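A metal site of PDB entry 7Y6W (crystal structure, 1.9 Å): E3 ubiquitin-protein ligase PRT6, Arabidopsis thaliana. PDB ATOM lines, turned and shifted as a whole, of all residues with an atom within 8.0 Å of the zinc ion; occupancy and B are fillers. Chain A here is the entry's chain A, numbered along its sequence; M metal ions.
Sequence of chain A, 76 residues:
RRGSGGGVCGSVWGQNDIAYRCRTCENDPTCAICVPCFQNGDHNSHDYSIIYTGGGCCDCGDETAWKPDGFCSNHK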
ATOM      1  N   ARG A  21     -22.454  20.766 -11.162  1.00  0.00           N
ATOM      2  CA  ARG A  21     -22.371  19.518 -11.904  1.00  0.00           C
ATOM      3  C   ARG A  21     -22.363  19.874 -13.380  1.00  0.00           C
ATOM      4  O   ARG A  21     -23.197  20.657 -13.827  1.00  0.00           O
ATOM      5  CB  ARG A  21     -23.575  18.627 -11.579  1.00  0.00           C
ATOM      6  CG  ARG A  21     -23.589  17.351 -12.405  1.00  0.00           C
ATOM      7  CD  ARG A  21     -24.441  16.250 -11.815  1.00  0.00           C
ATOM      8  NE  ARG A  21     -24.226  15.046 -12.611  1.00  0.00           N
ATOM      9  CZ  ARG A  21     -25.136  14.127 -12.870  1.00  0.00           C
ATOM     10  NH1 ARG A  21     -26.359  14.234 -12.358  1.00  0.00           N
ATOM     11  NH2 ARG A  21     -24.820  13.080 -13.645  1.00  0.00           N
ATOM     12  N   CYS A  22     -21.407  19.343 -14.135  1.00  0.00           N
ATOM     13  CA  CYS A  22     -21.468  19.502 -15.587  1.00  0.00           C
ATOM     14  C   CYS A  22     -21.439  18.128 -16.223  1.00  0.00           C
ATOM     15  O   CYS A  22     -20.409  17.450 -16.217  1.00  0.00           O
ATOM     16  CB  CYS A  22     -20.350  20.369 -16.147  1.00  0.00           C
ATOM     17  SG  CYS A  22     -20.590  20.616 -17.910  1.00  0.00           S
ATOM     18  N   ARG A  23     -22.568  17.719 -16.780  1.00  0.00           N
ATOM     19  CA  ARG A  23     -22.646  16.373 -17.342  1.00  0.00           C
ATOM     20  C   ARG A  23     -21.815  16.225 -18.597  1.00  0.00           C
ATOM     21  O   ARG A  23     -21.479  15.104 -18.972  1.00  0.00           O
ATOM     22  CB  ARG A  23     -24.121  16.014 -17.628  1.00  0.00           C
ATOM     23  CG  ARG A  23     -24.937  15.855 -16.360  1.00  0.00           C
ATOM     24  CD  ARG A  23     -26.421  16.051 -16.591  1.00  0.00           C
ATOM     25  NE  ARG A  23     -27.217  16.131 -15.352  1.00  0.00           N
ATOM     26  CZ  ARG A  23     -27.351  17.237 -14.633  1.00  0.00           C
ATOM     27  NH1 ARG A  23     -26.717  18.345 -15.000  1.00  0.00           N
ATOM     28  NH2 ARG A  23     -28.104  17.247 -13.538  1.00  0.00           N
ATOM     29  N   THR A  24     -21.475  17.329 -19.270  1.00  0.00           N
ATOM     30  CA  THR A  24     -20.620  17.262 -20.436  1.00  0.00           C
ATOM     31  C   THR A  24     -19.164  16.994 -20.059  1.00  0.00           C
ATOM     32  O   THR A  24     -18.466  16.260 -20.755  1.00  0.00           O
ATOM     33  CB  THR A  24     -20.741  18.554 -21.225  1.00  0.00           C
ATOM     34  OG1 THR A  24     -22.125  18.798 -21.495  1.00  0.00           O
ATOM     35  CG2 THR A  24     -19.948  18.474 -22.515  1.00  0.00           C
ATOM     36  N   CYS A  25     -18.701  17.586 -18.959  1.00  0.00           N
ATOM     37  CA  CYS A  25     -17.281  17.513 -18.593  1.00  0.00           C
ATOM     38  C   CYS A  25     -16.930  16.424 -17.594  1.00  0.00           C
ATOM     39  O   CYS A  25     -15.758  16.033 -17.516  1.00  0.00           O
ATOM     40  CB  CYS A  25     -16.848  18.877 -18.019  1.00  0.00           C
ATOM     41  SG  CYS A  25     -16.877  20.198 -19.206  1.00  0.00           S
ATOM     42  N   GLU A  26     -17.901  15.928 -16.820  1.00  0.00           N
ATOM     43  CA  GLU A  26     -17.611  14.992 -15.739  1.00  0.00           C
ATOM     44  C   GLU A  26     -17.129  13.638 -16.261  1.00  0.00           C
ATOM     45  O   GLU A  26     -17.556  13.158 -17.324  1.00  0.00           O
ATOM     46  CB  GLU A  26     -18.860  14.815 -14.877  1.00  0.00           C
ATOM     47  CG  GLU A  26     -19.947  13.969 -15.511  1.00  0.00           C
ATOM     48  CD  GLU A  26     -21.298  13.990 -14.773  1.00  0.00           C
ATOM     49  OE1 GLU A  26     -21.552  14.888 -13.950  1.00  0.00           O
ATOM     50  OE2 GLU A  26     -22.107  13.081 -15.038  1.00  0.00           O
ATOM     51  N   ILE A  33     -17.321  20.642  -9.805  1.00  0.00           N
ATOM     52  CA  ILE A  33     -16.305  21.686  -9.665  1.00  0.00           C
ATOM     53  C   ILE A  33     -16.862  22.891  -8.916  1.00  0.00           C
ATOM     54  O   ILE A  33     -18.067  23.164  -8.973  1.00  0.00           O
ATOM     55  CB  ILE A  33     -15.741  22.121 -11.031  1.00  0.00           C
ATOM     56  CG1 ILE A  33     -16.854  22.569 -11.970  1.00  0.00           C
ATOM     57  CG2 ILE A  33     -14.981  20.976 -11.696  1.00  0.00           C
ATOM     58  CD1 ILE A  33     -16.345  23.251 -13.206  1.00  0.00           C
ATOM     59  N   PHE A  38     -15.926  26.861 -12.250  1.00  0.00           N
ATOM     60  CA  PHE A  38     -16.926  26.851 -13.295  1.00  0.00           C
ATOM     61  C   PHE A  38     -16.920  28.187 -14.025  1.00  0.00           C
ATOM     62  O   PHE A  38     -16.895  28.216 -15.262  1.00  0.00           O
ATOM     63  CB  PHE A  38     -18.324  26.531 -12.723  1.00  0.00           C
ATOM     64  CG  PHE A  38     -19.417  26.474 -13.779  1.00  0.00           C
ATOM     65  CD1 PHE A  38     -19.702  25.318 -14.445  1.00  0.00           C
ATOM     66  CD2 PHE A  38     -20.106  27.613 -14.124  1.00  0.00           C
ATOM     67  CE1 PHE A  38     -20.663  25.265 -15.422  1.00  0.00           C
ATOM     68  CE2 PHE A  38     -21.084  27.581 -15.085  1.00  0.00           C
ATOM     69  CZ  PHE A  38     -21.367  26.399 -15.733  1.00  0.00           C
ATOM     70  N   GLY A  41     -14.057  28.743 -16.496  1.00  0.00           N
ATOM     71  CA  GLY A  41     -13.984  27.833 -17.620  1.00  0.00           C
ATOM     72  C   GLY A  41     -15.004  28.168 -18.697  1.00  0.00           C
ATOM     73  O   GLY A  41     -15.663  29.208 -18.689  1.00  0.00           O
ATOM     74  N   ASP A  42     -15.121  27.269 -19.659  1.00  0.00           N
ATOM     75  CA  ASP A  42     -16.091  27.448 -20.734  1.00  0.00           C
ATOM     76  C   ASP A  42     -17.011  26.234 -20.754  1.00  0.00           C
ATOM     77  O   ASP A  42     -16.586  25.152 -21.163  1.00  0.00           O
ATOM     78  CB  ASP A  42     -15.402  27.632 -22.082  1.00  0.00           C
ATOM     79  CG  ASP A  42     -16.388  27.790 -23.236  1.00  0.00           C
ATOM     80  OD1 ASP A  42     -15.996  28.425 -24.241  1.00  0.00           O
ATOM     81  OD2 ASP A  42     -17.536  27.287 -23.167  1.00  0.00           O
ATOM     82  N   HIS A  43     -18.256  26.425 -20.341  1.00  0.00           N
ATOM     83  CA  HIS A  43     -19.264  25.380 -20.393  1.00  0.00           C
ATOM     84  C   HIS A  43     -20.491  25.828 -21.178  1.00  0.00           C
ATOM     85  O   HIS A  43     -21.600  25.330 -20.951  1.00  0.00           O
ATOM     86  CB  HIS A  43     -19.650  24.951 -18.985  1.00  0.00           C
ATOM     87  CG  HIS A  43     -18.469  24.512 -18.180  1.00  0.00           C
ATOM     88  ND1 HIS A  43     -18.042  23.206 -18.154  1.00  0.00           N
ATOM     89  CD2 HIS A  43     -17.585  25.227 -17.457  1.00  0.00           C
ATOM     90  CE1 HIS A  43     -16.951  23.128 -17.409  1.00  0.00           C
ATOM     91  NE2 HIS A  43     -16.664  24.333 -16.971  1.00  0.00           N
ATOM     92  N   ASN A  44     -20.309  26.724 -22.128  1.00  0.00           N
ATOM     93  CA  ASN A  44     -21.463  27.196 -22.882  1.00  0.00           C
ATOM     94  C   ASN A  44     -21.990  26.065 -23.755  1.00  0.00           C
ATOM     95  O   ASN A  44     -21.231  25.405 -24.471  1.00  0.00           O
ATOM     96  CB  ASN A  44     -21.129  28.406 -23.725  1.00  0.00           C
ATOM     97  CG  ASN A  44     -22.367  29.017 -24.356  1.00  0.00           C
ATOM     98  OD1 ASN A  44     -23.241  29.534 -23.651  1.00  0.00           O
ATOM     99  ND2 ASN A  44     -22.474  28.941 -25.676  1.00  0.00           N
ATOM    100  N   SER A  45     -23.303  25.857 -23.707  1.00  0.00           N
ATOM    101  CA  SER A  45     -24.002  24.763 -24.359  1.00  0.00           C
ATOM    102  C   SER A  45     -23.708  23.417 -23.703  1.00  0.00           C
ATOM    103  O   SER A  45     -24.025  22.374 -24.292  1.00  0.00           O
ATOM    104  CB  SER A  45     -23.697  24.697 -25.852  1.00  0.00           C
ATOM    105  OG  SER A  45     -22.411  24.153 -26.085  1.00  0.00           O
ATOM    106  N   HIS A  46     -23.113  23.400 -22.511  1.00  0.00           N
ATOM    107  CA  HIS A  46     -22.948  22.175 -21.758  1.00  0.00           C
ATOM    108  C   HIS A  46     -24.193  21.932 -20.911  1.00  0.00           C
ATOM    109  O   HIS A  46     -24.959  22.850 -20.641  1.00  0.00           O
ATOM    110  CB  HIS A  46     -21.730  22.214 -20.832  1.00  0.00           C
ATOM    111  CG  HIS A  46     -20.413  22.178 -21.531  1.00  0.00           C
ATOM    112  ND1 HIS A  46     -19.235  21.877 -20.885  1.00  0.00           N
ATOM    113  CD2 HIS A  46     -20.066  22.450 -22.821  1.00  0.00           C
ATOM    114  CE1 HIS A  46     -18.225  21.905 -21.748  1.00  0.00           C
ATOM    115  NE2 HIS A  46     -18.698  22.292 -22.916  1.00  0.00           N
ATOM    116  N   ASP A  47     -24.350  20.704 -20.425  1.00  0.00           N
ATOM    117  CA  ASP A  47     -25.516  20.346 -19.618  1.00  0.00           C
ATOM    118  C   ASP A  47     -25.150  20.401 -18.139  1.00  0.00           C
ATOM    119  O   ASP A  47     -24.926  19.381 -17.492  1.00  0.00           O
ATOM    120  CB  ASP A  47     -26.049  18.977 -19.992  1.00  0.00           C
ATOM    121  CG  ASP A  47     -27.376  18.673 -19.280  1.00  0.00           C
ATOM    122  OD1 ASP A  47     -27.901  19.579 -18.589  1.00  0.00           O
ATOM    123  OD2 ASP A  47     -27.855  17.535 -19.396  1.00  0.00           O
ATOM    124  N   TYR A  48     -25.128  21.614 -17.579  1.00  0.00           N
ATOM    125  CA  TYR A  48     -24.699  21.796 -16.204  1.00  0.00           C
ATOM    126  C   TYR A  48     -25.868  22.214 -15.320  1.00  0.00           C
ATOM    127  O   TYR A  48     -26.889  22.702 -15.794  1.00  0.00           O
ATOM    128  CB  TYR A  48     -23.607  22.861 -16.111  1.00  0.00           C
ATOM    129  CG  TYR A  48     -24.028  24.193 -16.650  1.00  0.00           C
ATOM    130  CD1 TYR A  48     -24.723  25.107 -15.850  1.00  0.00           C
ATOM    131  CD2 TYR A  48     -23.727  24.556 -17.957  1.00  0.00           C
ATOM    132  CE1 TYR A  48     -25.110  26.336 -16.343  1.00  0.00           C
ATOM    133  CE2 TYR A  48     -24.097  25.803 -18.450  1.00  0.00           C
ATOM    134  CZ  TYR A  48     -24.778  26.684 -17.637  1.00  0.00           C
ATOM    135  OH  TYR A  48     -25.153  27.914 -18.143  1.00  0.00           O
ATOM    136  N   TRP A  66     -12.323  14.772 -14.484  1.00  0.00           N
ATOM    137  CA  TRP A  66     -12.937  15.892 -15.190  1.00  0.00           C
ATOM    138  C   TRP A  66     -12.223  15.989 -16.518  1.00  0.00           C
ATOM    139  O   TRP A  66     -11.000  15.856 -16.567  1.00  0.00           O
ATOM    140  CB  TRP A  66     -12.790  17.181 -14.380  1.00  0.00           C
ATOM    141  CG  TRP A  66     -13.746  18.255 -14.711  1.00  0.00           C
ATOM    142  CD1 TRP A  66     -13.513  19.322 -15.527  1.00  0.00           C
ATOM    143  CD2 TRP A  66     -15.090  18.386 -14.243  1.00  0.00           C
ATOM    144  NE1 TRP A  66     -14.623  20.120 -15.566  1.00  0.00           N
ATOM    145  CE2 TRP A  66     -15.617  19.551 -14.824  1.00  0.00           C
ATOM    146  CE3 TRP A  66     -15.900  17.631 -13.394  1.00  0.00           C
ATOM    147  CZ2 TRP A  66     -16.898  19.998 -14.566  1.00  0.00           C
ATOM    148  CZ3 TRP A  66     -17.165  18.057 -13.152  1.00  0.00           C
ATOM    149  CH2 TRP A  66     -17.657  19.244 -13.716  1.00  0.00           C
ATOM    150  N   LYS A  67     -12.985  16.196 -17.584  1.00  0.00           N
ATOM    151  CA  LYS A  67     -12.390  16.317 -18.905  1.00  0.00           C
ATOM    152  C   LYS A  67     -11.566  17.592 -19.014  1.00  0.00           C
ATOM    153  O   LYS A  67     -12.017  18.668 -18.559  1.00  0.00           O
ATOM    154  CB  LYS A  67     -13.483  16.279 -19.984  1.00  0.00           C
ATOM    155  CG  LYS A  67     -14.189  14.931 -20.035  1.00  0.00           C
ATOM    156  CD  LYS A  67     -15.430  14.936 -20.927  1.00  0.00           C
ATOM    157  CE  LYS A  67     -16.248  13.660 -20.780  1.00  0.00           C
ATOM    158  NZ  LYS A  67     -17.455  13.757 -21.676  1.00  0.00           N
ATOM    159  N   ASP A  69     -10.807  19.710 -21.311  1.00  0.00           N
ATOM    160  CA  ASP A  69     -11.386  20.891 -21.917  1.00  0.00           C
ATOM    161  C   ASP A  69     -12.316  21.621 -20.955  1.00  0.00           C
ATOM    162  O   ASP A  69     -12.742  22.740 -21.242  1.00  0.00           O
ATOM    163  CB  ASP A  69     -12.142  20.522 -23.195  1.00  0.00           C
ATOM    164  CG  ASP A  69     -13.146  19.373 -22.998  1.00  0.00           C
ATOM    165  OD1 ASP A  69     -12.738  18.192 -23.154  1.00  0.00           O
ATOM    166  OD2 ASP A  69     -14.329  19.647 -22.698  1.00  0.00           O
ATOM    167  N   GLY A  70     -12.667  21.002 -19.823  1.00  0.00           N
ATOM    168  CA  GLY A  70     -13.525  21.596 -18.828  1.00  0.00           C
ATOM    169  C   GLY A  70     -12.807  22.285 -17.705  1.00  0.00           C
ATOM    170  O   GLY A  70     -13.455  22.828 -16.815  1.00  0.00           O
ATOM    171  N   PHE A  71     -11.480  22.303 -17.738  1.00  0.00           N
ATOM    172  CA  PHE A  71     -10.712  22.941 -16.681  1.00  0.00           C
ATOM    173  C   PHE A  71     -10.815  24.450 -16.791  1.00  0.00           C
ATOM    174  O   PHE A  71     -11.006  25.014 -17.860  1.00  0.00           O
ATOM    175  CB  PHE A  71      -9.249  22.535 -16.756  1.00  0.00           C
ATOM    176  CG  PHE A  71      -8.992  21.094 -16.441  1.00  0.00           C
ATOM    177  CD1 PHE A  71      -7.720  20.558 -16.655  1.00  0.00           C
ATOM    178  CD2 PHE A  71      -9.994  20.272 -15.961  1.00  0.00           C
ATOM    179  CE1 PHE A  71      -7.468  19.233 -16.389  1.00  0.00           C
ATOM    180  CE2 PHE A  71      -9.741  18.967 -15.654  1.00  0.00           C
ATOM    181  CZ  PHE A  71      -8.493  18.442 -15.859  1.00  0.00           C
HETATM  182 ZN    ZN M   1     -18.782  21.508 -18.952  1.00  0.00          ZN
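The zinc ion is bound by a ring nitrogen (ND1) of His 43, a ring nitrogen (ND1) of His 46, the side-chain sulfur (SG) of Cys 22 and the side-chain sulfur (SG) of Cys 25. The zinc ion has four donor atoms within binding distance.
Within 4 Å of the zinc ion: Cys 22, Cys 25, His 43 and His 46. The nearest printed residue that does not touch the zinc ion is Thr 24 (4.2 Å).
The backbone NH (N) of Thr 24 sits close to the side-chain sulfur (SG) of Cys 22 (3.7 Å). The backbone NH of Lys 67 sits at hydrogen-bond distance from the backbone carbonyl oxygen of Cys 25 (2.8 Å).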
